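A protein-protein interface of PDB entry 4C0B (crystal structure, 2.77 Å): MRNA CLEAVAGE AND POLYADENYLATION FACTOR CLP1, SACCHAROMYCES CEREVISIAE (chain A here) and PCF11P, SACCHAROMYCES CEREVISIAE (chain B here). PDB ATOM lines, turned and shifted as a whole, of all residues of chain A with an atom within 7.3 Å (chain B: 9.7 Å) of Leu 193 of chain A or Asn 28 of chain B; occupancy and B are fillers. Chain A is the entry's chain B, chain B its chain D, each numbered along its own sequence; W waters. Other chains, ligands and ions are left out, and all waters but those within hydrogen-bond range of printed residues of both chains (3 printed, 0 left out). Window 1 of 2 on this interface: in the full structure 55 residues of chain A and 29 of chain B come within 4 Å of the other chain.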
ATOM      1  N   PHE A 167      -6.644   0.443  13.226  1.00  0.00           N
ATOM      2  CA  PHE A 167      -7.382   1.455  14.032  1.00  0.00           C
ATOM      3  C   PHE A 167      -8.890   1.200  14.165  1.00  0.00           C
ATOM      4  O   PHE A 167      -9.586   1.959  14.853  1.00  0.00           O
ATOM      5  CB  PHE A 167      -7.118   2.912  13.549  1.00  0.00           C
ATOM      6  CG  PHE A 167      -5.671   3.342  13.482  1.00  0.00           C
ATOM      7  CD1 PHE A 167      -4.905   3.447  14.636  1.00  0.00           C
ATOM      8  CD2 PHE A 167      -5.080   3.656  12.269  1.00  0.00           C
ATOM      9  CE1 PHE A 167      -3.581   3.882  14.578  1.00  0.00           C
ATOM     10  CE2 PHE A 167      -3.745   4.081  12.207  1.00  0.00           C
ATOM     11  CZ  PHE A 167      -3.016   4.203  13.363  1.00  0.00           C
ATOM     12  N   GLN A 191      -5.250   2.430  18.574  1.00  0.00           N
ATOM     13  CA  GLN A 191      -6.705   2.435  18.676  1.00  0.00           C
ATOM     14  C   GLN A 191      -7.348   3.801  18.638  1.00  0.00           C
ATOM     15  O   GLN A 191      -6.646   4.803  18.715  1.00  0.00           O
ATOM     16  CB  GLN A 191      -7.189   1.548  19.820  1.00  0.00           C
ATOM     17  CG  GLN A 191      -6.669   1.906  21.191  1.00  0.00           C
ATOM     18  CD  GLN A 191      -6.834   0.759  22.142  1.00  0.00           C
ATOM     19  OE1 GLN A 191      -7.814   0.682  22.907  1.00  0.00           O
ATOM     20  NE2 GLN A 191      -5.848  -0.129  22.140  1.00  0.00           N
ATOM     21  N   SER A 192      -8.670   3.846  18.423  1.00  0.00           N
ATOM     22  CA  SER A 192      -9.416   5.101  18.345  1.00  0.00           C
ATOM     23  C   SER A 192      -9.690   5.721  19.729  1.00  0.00           C
ATOM     24  O   SER A 192      -9.377   5.097  20.732  1.00  0.00           O
ATOM     25  CB  SER A 192     -10.663   4.979  17.465  1.00  0.00           C
ATOM     26  OG  SER A 192     -11.448   3.813  17.630  1.00  0.00           O
ATOM     27  N   LEU A 193     -10.195   6.971  19.778  1.00  0.00           N
ATOM     28  CA  LEU A 193     -10.471   7.656  21.035  1.00  0.00           C
ATOM     29  C   LEU A 193     -11.340   6.899  22.010  1.00  0.00           C
ATOM     30  O   LEU A 193     -12.229   6.135  21.605  1.00  0.00           O
ATOM     31  CB  LEU A 193     -11.017   9.071  20.822  1.00  0.00           C
ATOM     32  CG  LEU A 193     -10.168  10.031  19.968  1.00  0.00           C
ATOM     33  CD1 LEU A 193     -10.753  11.417  19.962  1.00  0.00           C
ATOM     34  CD2 LEU A 193      -8.732  10.092  20.443  1.00  0.00           C
ATOM     35  N   THR A 194     -11.028   7.088  23.310  1.00  0.00           N
ATOM     36  CA  THR A 194     -11.725   6.497  24.458  1.00  0.00           C
ATOM     37  C   THR A 194     -12.234   7.635  25.371  1.00  0.00           C
ATOM     38  O   THR A 194     -11.853   8.796  25.196  1.00  0.00           O
ATOM     39  CB  THR A 194     -10.838   5.475  25.187  1.00  0.00           C
ATOM     40  OG1 THR A 194      -9.758   6.167  25.809  1.00  0.00           O
ATOM     41  CG2 THR A 194     -10.288   4.409  24.259  1.00  0.00           C
ATOM     42  N   SER A 195     -13.094   7.301  26.331  1.00  0.00           N
ATOM     43  CA  SER A 195     -13.717   8.263  27.238  1.00  0.00           C
ATOM     44  C   SER A 195     -12.822   8.770  28.390  1.00  0.00           C
ATOM     45  O   SER A 195     -13.241   9.663  29.111  1.00  0.00           O
ATOM     46  CB  SER A 195     -15.024   7.693  27.782  1.00  0.00           C
ATOM     47  OG  SER A 195     -14.766   6.513  28.523  1.00  0.00           O
ATOM     48  N   GLY A 196     -11.618   8.241  28.557  1.00  0.00           N
ATOM     49  CA  GLY A 196     -10.772   8.700  29.650  1.00  0.00           C
ATOM     50  C   GLY A 196      -9.285   8.823  29.360  1.00  0.00           C
ATOM     51  O   GLY A 196      -8.866   9.159  28.241  1.00  0.00           O
ATOM     52  N   THR A 198      -5.386   7.571  28.948  1.00  0.00           N
ATOM     53  CA  THR A 198      -4.613   6.498  28.301  1.00  0.00           C
ATOM     54  C   THR A 198      -3.113   6.830  28.336  1.00  0.00           C
ATOM     55  O   THR A 198      -2.756   8.011  28.399  1.00  0.00           O
ATOM     56  CB  THR A 198      -5.112   6.270  26.846  1.00  0.00           C
ATOM     57  OG1 THR A 198      -5.089   7.499  26.106  1.00  0.00           O
ATOM     58  CG2 THR A 198      -6.510   5.671  26.782  1.00  0.00           C
ATOM     59  N   HIS A 201      -1.638   8.750  23.232  1.00  0.00           N
ATOM     60  CA  HIS A 201      -2.705   9.531  22.598  1.00  0.00           C
ATOM     61  C   HIS A 201      -3.214   8.620  21.468  1.00  0.00           C
ATOM     62  O   HIS A 201      -2.419   8.114  20.677  1.00  0.00           O
ATOM     63  CB  HIS A 201      -2.207  10.867  22.016  1.00  0.00           C
ATOM     64  CG  HIS A 201      -1.733  11.840  23.045  1.00  0.00           C
ATOM     65  ND1 HIS A 201      -0.395  12.250  23.102  1.00  0.00           N
ATOM     66  CD2 HIS A 201      -2.425  12.467  24.023  1.00  0.00           C
ATOM     67  CE1 HIS A 201      -0.334  13.107  24.106  1.00  0.00           C
ATOM     68  NE2 HIS A 201      -1.528  13.269  24.693  1.00  0.00           N
ATOM     69  N   ASN A 202      -4.512   8.337  21.474  1.00  0.00           N
ATOM     70  CA  ASN A 202      -5.181   7.482  20.517  1.00  0.00           C
ATOM     71  C   ASN A 202      -5.556   8.283  19.295  1.00  0.00           C
ATOM     72  O   ASN A 202      -5.457   9.513  19.282  1.00  0.00           O
ATOM     73  CB  ASN A 202      -6.423   6.876  21.164  1.00  0.00           C
ATOM     74  CG  ASN A 202      -6.151   6.017  22.361  1.00  0.00           C
ATOM     75  OD1 ASN A 202      -5.189   5.258  22.415  1.00  0.00           O
ATOM     76  ND2 ASN A 202      -7.010   6.123  23.335  1.00  0.00           N
ATOM     77  N   LYS A 203      -6.025   7.584  18.278  1.00  0.00           N
ATOM     78  CA  LYS A 203      -6.370   8.133  16.974  1.00  0.00           C
ATOM     79  C   LYS A 203      -7.862   8.456  16.758  1.00  0.00           C
ATOM     80  O   LYS A 203      -8.739   7.917  17.445  1.00  0.00           O
ATOM     81  CB  LYS A 203      -5.816   7.162  15.914  1.00  0.00           C
ATOM     82  CG  LYS A 203      -4.439   7.568  15.417  1.00  0.00           C
ATOM     83  CD  LYS A 203      -3.297   7.096  16.266  1.00  0.00           C
ATOM     84  CE  LYS A 203      -2.122   8.021  16.156  1.00  0.00           C
ATOM     85  NZ  LYS A 203      -1.232   7.835  17.322  1.00  0.00           N
ATOM     86  N   GLN A 204      -8.142   9.354  15.812  1.00  0.00           N
ATOM     87  CA  GLN A 204      -9.499   9.769  15.451  1.00  0.00           C
ATOM     88  C   GLN A 204      -9.718   9.447  13.957  1.00  0.00           C
ATOM     89  O   GLN A 204      -9.490  10.307  13.089  1.00  0.00           O
ATOM     90  CB  GLN A 204      -9.755  11.253  15.822  1.00  0.00           C
ATOM     91  CG  GLN A 204     -11.135  11.791  15.438  1.00  0.00           C
ATOM     92  CD  GLN A 204     -12.197  11.381  16.415  1.00  0.00           C
ATOM     93  OE1 GLN A 204     -12.644  10.225  16.456  1.00  0.00           O
ATOM     94  NE2 GLN A 204     -12.563  12.299  17.277  1.00  0.00           N
ATOM     95  N   PRO A 205     -10.137   8.190  13.645  1.00  0.00           N
ATOM     96  CA  PRO A 205     -10.276   7.788  12.239  1.00  0.00           C
ATOM     97  C   PRO A 205     -11.595   8.081  11.534  1.00  0.00           C
ATOM     98  O   PRO A 205     -12.636   8.187  12.175  1.00  0.00           O
ATOM     99  CB  PRO A 205     -10.043   6.264  12.300  1.00  0.00           C
ATOM    100  CG  PRO A 205     -10.576   5.842  13.616  1.00  0.00           C
ATOM    101  CD  PRO A 205     -10.376   7.036  14.551  1.00  0.00           C
ATOM    102  N   TYR A 332     -11.742  -3.556  19.769  1.00  0.00           N
ATOM    103  CA  TYR A 332     -12.718  -2.491  19.536  1.00  0.00           C
ATOM    104  C   TYR A 332     -13.578  -2.232  20.764  1.00  0.00           C
ATOM    105  O   TYR A 332     -13.758  -1.067  21.128  1.00  0.00           O
ATOM    106  CB  TYR A 332     -13.625  -2.795  18.322  1.00  0.00           C
ATOM    107  CG  TYR A 332     -14.649  -1.712  18.051  1.00  0.00           C
ATOM    108  CD1 TYR A 332     -14.275  -0.495  17.483  1.00  0.00           C
ATOM    109  CD2 TYR A 332     -15.996  -1.896  18.372  1.00  0.00           C
ATOM    110  CE1 TYR A 332     -15.206   0.521  17.263  1.00  0.00           C
ATOM    111  CE2 TYR A 332     -16.946  -0.900  18.121  1.00  0.00           C
ATOM    112  CZ  TYR A 332     -16.542   0.307  17.565  1.00  0.00           C
ATOM    113  OH  TYR A 332     -17.435   1.323  17.349  1.00  0.00           O
ATOM    114  N   LEU A 341     -11.064  -1.453  28.458  1.00  0.00           N
ATOM    115  CA  LEU A 341     -12.301  -0.706  28.222  1.00  0.00           C
ATOM    116  C   LEU A 341     -13.524  -1.496  28.661  1.00  0.00           C
ATOM    117  O   LEU A 341     -13.481  -2.732  28.718  1.00  0.00           O
ATOM    118  CB  LEU A 341     -12.438  -0.229  26.761  1.00  0.00           C
ATOM    119  CG  LEU A 341     -11.255   0.553  26.166  1.00  0.00           C
ATOM    120  CD1 LEU A 341     -11.515   0.870  24.761  1.00  0.00           C
ATOM    121  CD2 LEU A 341     -10.972   1.820  26.926  1.00  0.00           C
ATOM    122  N   LEU A 406     -21.179   5.558  12.644  1.00  0.00           N
ATOM    123  CA  LEU A 406     -21.107   5.953  14.052  1.00  0.00           C
ATOM    124  C   LEU A 406     -20.204   4.972  14.838  1.00  0.00           C
ATOM    125  O   LEU A 406     -19.397   5.390  15.665  1.00  0.00           O
ATOM    126  CB  LEU A 406     -22.537   5.955  14.619  1.00  0.00           C
ATOM    127  CG  LEU A 406     -22.748   6.378  16.047  1.00  0.00           C
ATOM    128  CD1 LEU A 406     -22.669   7.863  16.191  1.00  0.00           C
ATOM    129  CD2 LEU A 406     -24.103   5.927  16.500  1.00  0.00           C
ATOM    130  N   GLY A 407     -20.331   3.684  14.532  1.00  0.00           N
ATOM    131  CA  GLY A 407     -19.575   2.632  15.185  1.00  0.00           C
ATOM    132  C   GLY A 407     -20.091   1.259  14.824  1.00  0.00           C
ATOM    133  O   GLY A 407     -20.771   1.089  13.811  1.00  0.00           O
ATOM    134  N   PRO A 426     -20.061  -0.387  22.065  1.00  0.00           N
ATOM    135  CA  PRO A 426     -18.775   0.103  22.588  1.00  0.00           C
ATOM    136  C   PRO A 426     -19.012   1.184  23.661  1.00  0.00           C
ATOM    137  O   PRO A 426     -18.221   1.311  24.604  1.00  0.00           O
ATOM    138  CB  PRO A 426     -18.091   0.680  21.339  1.00  0.00           C
ATOM    139  CG  PRO A 426     -19.166   1.047  20.420  1.00  0.00           C
ATOM    140  CD  PRO A 426     -20.339   0.164  20.714  1.00  0.00           C
ATOM    141  N   VAL A 427     -20.147   1.930  23.528  1.00  0.00           N
ATOM    142  CA  VAL A 427     -20.578   3.059  24.354  1.00  0.00           C
ATOM    143  C   VAL A 427     -21.734   2.714  25.318  1.00  0.00           C
ATOM    144  O   VAL A 427     -22.808   2.321  24.854  1.00  0.00           O
ATOM    145  CB  VAL A 427     -20.933   4.298  23.473  1.00  0.00           C
ATOM    146  CG1 VAL A 427     -21.252   5.509  24.328  1.00  0.00           C
ATOM    147  CG2 VAL A 427     -19.822   4.620  22.481  1.00  0.00           C
ATOM    148  N   GLN B  25     -13.813   3.288  31.773  1.00  0.00           N
ATOM    149  CA  GLN B  25     -13.604   4.017  30.520  1.00  0.00           C
ATOM    150  C   GLN B  25     -14.125   3.177  29.335  1.00  0.00           C
ATOM    151  O   GLN B  25     -14.023   1.941  29.366  1.00  0.00           O
ATOM    152  CB  GLN B  25     -12.119   4.286  30.386  1.00  0.00           C
ATOM    153  CG  GLN B  25     -11.649   4.883  29.102  1.00  0.00           C
ATOM    154  CD  GLN B  25     -10.182   5.139  29.149  1.00  0.00           C
ATOM    155  OE1 GLN B  25      -9.667   5.941  28.395  1.00  0.00           O
ATOM    156  NE2 GLN B  25      -9.479   4.485  30.032  1.00  0.00           N
ATOM    157  N   SER B  26     -14.651   3.839  28.279  1.00  0.00           N
ATOM    158  CA  SER B  26     -15.190   3.114  27.132  1.00  0.00           C
ATOM    159  C   SER B  26     -14.720   3.675  25.789  1.00  0.00           C
ATOM    160  O   SER B  26     -14.267   4.811  25.742  1.00  0.00           O
ATOM    161  CB  SER B  26     -16.715   3.112  27.186  1.00  0.00           C
ATOM    162  OG  SER B  26     -17.196   2.634  28.430  1.00  0.00           O
ATOM    163  N   ARG B  27     -14.869   2.891  24.701  1.00  0.00           N
ATOM    164  CA  ARG B  27     -14.582   3.292  23.330  1.00  0.00           C
ATOM    165  C   ARG B  27     -15.587   4.383  22.934  1.00  0.00           C
ATOM    166  O   ARG B  27     -16.744   4.318  23.346  1.00  0.00           O
ATOM    167  CB  ARG B  27     -14.765   2.073  22.407  1.00  0.00           C
ATOM    168  CG  ARG B  27     -14.608   2.312  20.899  1.00  0.00           C
ATOM    169  CD  ARG B  27     -13.183   2.459  20.460  1.00  0.00           C
ATOM    170  NE  ARG B  27     -12.403   1.279  20.832  1.00  0.00           N
ATOM    171  CZ  ARG B  27     -11.154   1.311  21.279  1.00  0.00           C
ATOM    172  NH1 ARG B  27     -10.520   2.467  21.417  1.00  0.00           N
ATOM    173  NH2 ARG B  27     -10.540   0.192  21.620  1.00  0.00           N
ATOM    174  N   ASN B  28     -15.164   5.367  22.130  1.00  0.00           N
ATOM    175  CA  ASN B  28     -16.058   6.420  21.671  1.00  0.00           C
ATOM    176  C   ASN B  28     -16.676   6.112  20.302  1.00  0.00           C
ATOM    177  O   ASN B  28     -16.114   5.351  19.517  1.00  0.00           O
ATOM    178  CB  ASN B  28     -15.300   7.721  21.566  1.00  0.00           C
ATOM    179  CG  ASN B  28     -14.988   8.408  22.847  1.00  0.00           C
ATOM    180  OD1 ASN B  28     -15.301   7.943  23.938  1.00  0.00           O
ATOM    181  ND2 ASN B  28     -14.347   9.546  22.717  1.00  0.00           N
ATOM    182  N   TRP B  29     -17.811   6.757  19.993  1.00  0.00           N
ATOM    183  CA  TRP B  29     -18.431   6.646  18.680  1.00  0.00           C
ATOM    184  C   TRP B  29     -17.562   7.499  17.725  1.00  0.00           C
ATOM    185  O   TRP B  29     -16.831   8.414  18.166  1.00  0.00           O
ATOM    186  CB  TRP B  29     -19.835   7.268  18.713  1.00  0.00           C
ATOM    187  CG  TRP B  29     -20.866   6.566  19.538  1.00  0.00           C
ATOM    188  CD1 TRP B  29     -21.673   7.138  20.467  1.00  0.00           C
ATOM    189  CD2 TRP B  29     -21.349   5.216  19.364  1.00  0.00           C
ATOM    190  NE1 TRP B  29     -22.605   6.230  20.913  1.00  0.00           N
ATOM    191  CE2 TRP B  29     -22.434   5.044  20.249  1.00  0.00           C
ATOM    192  CE3 TRP B  29     -20.966   4.130  18.545  1.00  0.00           C
ATOM    193  CZ2 TRP B  29     -23.098   3.818  20.393  1.00  0.00           C
ATOM    194  CZ3 TRP B  29     -21.646   2.923  18.669  1.00  0.00           C
ATOM    195  CH2 TRP B  29     -22.687   2.772  19.594  1.00  0.00           C
ATOM    196  N   TYR B  30     -17.649   7.227  16.421  1.00  0.00           N
ATOM    197  CA  TYR B  30     -16.886   7.980  15.430  1.00  0.00           C
ATOM    198  C   TYR B  30     -17.589   9.316  15.143  1.00  0.00           C
ATOM    199  O   TYR B  30     -18.760   9.506  15.524  1.00  0.00           O
ATOM    200  CB  TYR B  30     -16.683   7.122  14.160  1.00  0.00           C
ATOM    201  CG  TYR B  30     -15.864   5.852  14.370  1.00  0.00           C
ATOM    202  CD1 TYR B  30     -14.654   5.885  15.054  1.00  0.00           C
ATOM    203  CD2 TYR B  30     -16.286   4.624  13.854  1.00  0.00           C
ATOM    204  CE1 TYR B  30     -13.896   4.730  15.243  1.00  0.00           C
ATOM    205  CE2 TYR B  30     -15.535   3.452  14.044  1.00  0.00           C
ATOM    206  CZ  TYR B  30     -14.332   3.513  14.728  1.00  0.00           C
ATOM    207  OH  TYR B  30     -13.569   2.377  14.959  1.00  0.00           O
ATOM    208  N   LEU B  31     -16.843  10.280  14.553  1.00  0.00           N
ATOM    209  CA  LEU B  31     -17.379  11.593  14.162  1.00  0.00           C
ATOM    210  C   LEU B  31     -18.009  11.483  12.773  1.00  0.00           C
ATOM    211  O   LEU B  31     -17.678  10.558  12.009  1.00  0.00           O
ATOM    212  CB  LEU B  31     -16.284  12.667  14.135  1.00  0.00           C
ATOM    213  CG  LEU B  31     -15.553  13.044  15.452  1.00  0.00           C
ATOM    214  CD1 LEU B  31     -14.513  14.106  15.178  1.00  0.00           C
ATOM    215  CD2 LEU B  31     -16.448  13.619  16.429  1.00  0.00           C
ATOM    216  N   TRP B  36     -15.604  15.416  11.448  1.00  0.00           N
ATOM    217  CA  TRP B  36     -14.274  14.865  11.246  1.00  0.00           C
ATOM    218  C   TRP B  36     -13.414  15.794  10.394  1.00  0.00           C
ATOM    219  O   TRP B  36     -12.285  16.046  10.758  1.00  0.00           O
ATOM    220  CB  TRP B  36     -14.335  13.443  10.684  1.00  0.00           C
ATOM    221  CG  TRP B  36     -12.999  12.788  10.536  1.00  0.00           C
ATOM    222  CD1 TRP B  36     -12.288  12.142  11.505  1.00  0.00           C
ATOM    223  CD2 TRP B  36     -12.189  12.755   9.349  1.00  0.00           C
ATOM    224  NE1 TRP B  36     -11.103  11.667  10.986  1.00  0.00           N
ATOM    225  CE2 TRP B  36     -11.001  12.057   9.672  1.00  0.00           C
ATOM    226  CE3 TRP B  36     -12.386  13.176   8.018  1.00  0.00           C
ATOM    227  CZ2 TRP B  36     -10.004  11.800   8.730  1.00  0.00           C
ATOM    228  CZ3 TRP B  36     -11.370  12.958   7.098  1.00  0.00           C
ATOM    229  CH2 TRP B  36     -10.195  12.283   7.460  1.00  0.00           C
ATOM    230  N   PHE B  39     -12.264  18.658  12.466  1.00  0.00           N
ATOM    231  CA  PHE B  39     -11.483  18.226  13.625  1.00  0.00           C
ATOM    232  C   PHE B  39     -10.016  18.470  13.466  1.00  0.00           C
ATOM    233  O   PHE B  39      -9.470  18.326  12.365  1.00  0.00           O
ATOM    234  CB  PHE B  39     -11.738  16.737  13.935  1.00  0.00           C
ATOM    235  CG  PHE B  39     -11.194  16.228  15.252  1.00  0.00           C
ATOM    236  CD1 PHE B  39     -11.884  16.445  16.442  1.00  0.00           C
ATOM    237  CD2 PHE B  39      -9.990  15.511  15.303  1.00  0.00           C
ATOM    238  CE1 PHE B  39     -11.376  15.968  17.662  1.00  0.00           C
ATOM    239  CE2 PHE B  39      -9.480  15.040  16.530  1.00  0.00           C
ATOM    240  CZ  PHE B  39     -10.174  15.280  17.704  1.00  0.00           C
ATOM    241  N   LYS B  40      -9.369  18.844  14.591  1.00  0.00           N
ATOM    242  CA  LYS B  40      -7.937  19.106  14.699  1.00  0.00           C
ATOM    243  C   LYS B  40      -7.361  18.182  15.762  1.00  0.00           C
ATOM    244  O   LYS B  40      -7.770  18.213  16.921  1.00  0.00           O
ATOM    245  CB  LYS B  40      -7.669  20.577  15.030  1.00  0.00           C
ATOM    246  CG  LYS B  40      -8.320  21.589  14.067  1.00  0.00           C
ATOM    247  CD  LYS B  40      -7.599  21.771  12.714  1.00  0.00           C
ATOM    248  CE  LYS B  40      -8.293  22.757  11.794  1.00  0.00           C
ATOM    249  NZ  LYS B  40      -9.623  22.293  11.369  1.00  0.00           N
ATOM    250  N   ASP B  41      -6.422  17.321  15.346  1.00  0.00           N
ATOM    251  CA  ASP B  41      -5.790  16.325  16.206  1.00  0.00           C
ATOM    252  C   ASP B  41      -5.009  16.909  17.405  1.00  0.00           C
ATOM    253  O   ASP B  41      -4.746  16.168  18.352  1.00  0.00           O
ATOM    254  CB  ASP B  41      -5.038  15.272  15.386  1.00  0.00           C
ATOM    255  CG  ASP B  41      -5.864  14.075  14.906  1.00  0.00           C
ATOM    256  OD1 ASP B  41      -7.032  14.280  14.450  1.00  0.00           O
ATOM    257  OD2 ASP B  41      -5.341  12.936  14.952  1.00  0.00           O
ATOM    258  N   ASP B  42      -4.776  18.252  17.442  1.00  0.00           N
ATOM    259  CA  ASP B  42      -4.157  18.967  18.582  1.00  0.00           C
ATOM    260  C   ASP B  42      -5.081  18.922  19.795  1.00  0.00           C
ATOM    261  O   ASP B  42      -4.613  19.125  20.918  1.00  0.00           O
ATOM    262  CB  ASP B  42      -3.773  20.424  18.244  1.00  0.00           C
ATOM    263  CG  ASP B  42      -2.646  20.612  17.214  1.00  0.00           C
ATOM    264  OD1 ASP B  42      -1.998  19.590  16.824  1.00  0.00           O
ATOM    265  OD2 ASP B  42      -2.439  21.769  16.765  1.00  0.00           O
ATOM    266  N   GLU B  43      -6.393  18.617  19.572  1.00  0.00           N
ATOM    267  CA  GLU B  43      -7.391  18.402  20.623  1.00  0.00           C
ATOM    268  C   GLU B  43      -6.961  17.166  21.440  1.00  0.00           C
ATOM    269  O   GLU B  43      -7.118  17.156  22.653  1.00  0.00           O
ATOM    270  CB  GLU B  43      -8.778  18.166  20.019  1.00  0.00           C
ATOM    271  CG  GLU B  43      -9.630  19.413  19.870  1.00  0.00           C
ATOM    272  CD  GLU B  43     -11.110  19.112  19.702  1.00  0.00           C
ATOM    273  OE1 GLU B  43     -11.750  18.704  20.704  1.00  0.00           O
ATOM    274  OE2 GLU B  43     -11.638  19.325  18.584  1.00  0.00           O
ATOM    275  N   ILE B  44      -6.394  16.143  20.770  1.00  0.00           N
ATOM    276  CA  ILE B  44      -5.877  14.921  21.404  1.00  0.00           C
ATOM    277  C   ILE B  44      -4.460  15.241  21.951  1.00  0.00           C
ATOM    278  O   ILE B  44      -4.285  15.272  23.169  1.00  0.00           O
ATOM    279  CB  ILE B  44      -5.889  13.686  20.435  1.00  0.00           C
ATOM    280  CG1 ILE B  44      -7.230  13.565  19.636  1.00  0.00           C
ATOM    281  CG2 ILE B  44      -5.539  12.385  21.187  1.00  0.00           C
ATOM    282  CD1 ILE B  44      -7.127  12.749  18.296  1.00  0.00           C
ATOM    283  N   THR B  45      -3.482  15.525  21.028  1.00  0.00           N
ATOM    284  CA  THR B  45      -2.063  15.895  21.195  1.00  0.00           C
ATOM    285  C   THR B  45      -1.706  16.691  22.478  1.00  0.00           C
ATOM    286  O   THR B  45      -0.578  16.577  22.969  1.00  0.00           O
ATOM    287  CB  THR B  45      -1.577  16.513  19.864  1.00  0.00           C
ATOM    288  OG1 THR B  45      -1.486  15.468  18.906  1.00  0.00           O
ATOM    289  CG2 THR B  45      -0.232  17.232  19.953  1.00  0.00           C
ATOM    290  N   THR B  47      -3.922  17.116  26.056  1.00  0.00           N
ATOM    291  CA  THR B  47      -3.022  15.958  26.284  1.00  0.00           C
ATOM    292  C   THR B  47      -3.805  14.652  26.534  1.00  0.00           C
ATOM    293  O   THR B  47      -4.867  14.426  25.952  1.00  0.00           O
ATOM    294  CB  THR B  47      -1.958  16.213  27.382  1.00  0.00           C
ATOM    295  OG1 THR B  47      -0.966  15.183  27.312  1.00  0.00           O
ATOM    296  CG2 THR B  47      -2.555  16.279  28.798  1.00  0.00           C
HETATM  297  O   HOH W   1     -16.759   3.758  17.507  1.00  0.00           O
HETATM  298  O   HOH W   2     -13.482   5.456  19.068  1.00  0.00           O
HETATM  299  O   HOH W   3      -5.961  10.542  14.378  1.00  0.00           O
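Water W1 lies within hydrogen-bond range of OH of Tyr 332 of chain A and O of Asn 28 of chain B. Water W3 bridges OD2 of Asp 41 of chain B (2.5 Å) and N of Gln 204 of chain A (2.9 Å). Water W2 lies within hydrogen-bond range of the backbone carbonyl oxygen (O) of Asn 28 of chain B (2.7 Å), the backbone carbonyl oxygen (O) of Leu 193 of chain A (2.9 Å) and the side-chain hydroxyl (OG) of Ser 192 of chain A (3.0 Å).
The backbone carbonyl oxygen (O) of Gln 191 of chain A sits at hydrogen-bond distance from the backbone NH (N) of Lys 203 of chain A (2.9 Å). O of Lys 203 of chain A lies within hydrogen-bond range of N of Leu 193 of chain A (2.9 Å). OG1 of Thr 45 of chain B lies within hydrogen-bond range of O of Asp 41 of chain B.
The guanidinium group (NH2) of Arg 27 of chain B is in hydrogen-bond range of the side-chain amide oxygen (OE1) of Gln 191 of chain A, at 3.1 Å. The backbone carbonyl oxygen (O) of Ser 192 of chain A is in hydrogen-bond range of the guanidinium group (NH1) of Arg 27 of chain B (2.9 Å). The backbone carbonyl oxygen of Leu 193 of chain A sits at hydrogen-bond distance from the backbone NH of Asn 28 of chain B (3.1 Å). OG1 of Thr 194 of chain A sits at hydrogen-bond distance from OE1 of Gln 25 of chain B, 2.6 Å away. The side-chain hydroxyl (OG) of Ser 195 of chain A sits at hydrogen-bond distance from the backbone NH (N) of Ser 26 of chain B, at 2.7 Å. The backbone NH of Ser 195 of chain A sits at hydrogen-bond distance from the side-chain amide oxygen of Asn 28 of chain B (3.3 Å). The side-chain amide oxygen (OE1) of Gln 25 of chain B is in hydrogen-bond range of the backbone NH (N) of Gly 196 of chain A, at 3.0 Å. A ring nitrogen (NE2) of His 201 of chain A lies close to the side-chain hydroxyl of Thr 47 of chain B (3.3 Å). O of Gln 204 of chain A sits at hydrogen-bond distance from NE1 of Trp 36 of chain B, at 3.0 Å. The backbone carbonyl oxygen (O) of Tyr 332 of chain A lies within hydrogen-bond range of the guanidinium group (NE) of Arg 27 of chain B. The backbone carbonyl oxygen of Leu 406 of chain A lies within hydrogen-bond range of the backbone NH of Tyr 30 of chain B (2.6 Å).
Printed residues of chain B within 4 Å of Gln 191 of chain A: Arg 27. Printed residues of chain B within 4 Å of Leu 193 of chain A: Arg 27, Asn 28 and Ile 44. Printed residues of chain A within 4 Å of Gln 25 of chain B: Thr 194 (2.6 Å), Ser 195 (3.4 Å), Gly 196 (3.0 Å), Thr 198 (3.6 Å) and Leu 341 (3.4 Å). Of the printed residues of chain A, Asn 28 of chain B touches Leu 193, Thr 194 and Ser 195.
Of the 19 printed residues of chain A, 17 touch a printed residue of chain B. Hydrophobic or aromatic side chains of chain A within 4 Å of the printed part of chain B: Leu 193, His 201, Pro 205, Tyr 332, Leu 341, Leu 406, Pro 426 and Val 427. Of the 16 printed residues of chain B, 12 touch a printed residue of chain A. Hydrophobic or aromatic side chains of chain B that line the printed part of chain A: Trp 29, Tyr 30, Leu 31, Trp 36, Phe 39 and Ile 44. Among the printed residues, 37 pairs touch across the chains. Among the printed residues, no Asp or Glu carboxylate lies within 4 Å of a Lys or Arg side-chain nitrogen of the other chain.
Ser 192 of chain A touches Tyr 30 of chain B. Asn 28 of chain B touches Thr 194 of chain A (OD1 to C, 3.4 Å). Asn 202 of chain A touches Ile 44 of chain B (O to CG2, 3.4 Å). Gln 204 of chain A touches Ile 44 of chain B (CB to CD1, 3.9 Å). Pro 205 of chain A touches Trp 36 of chain B. O of Gln 25 of chain B touches CA of Leu 341 of chain A, 3.4 Å away. Trp 29 of chain B touches Leu 406 of chain A (CA to O, 3.4 Å). Gly 407 of chain A touches Trp 29 of chain B (CA to CE3, 3.9 Å).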
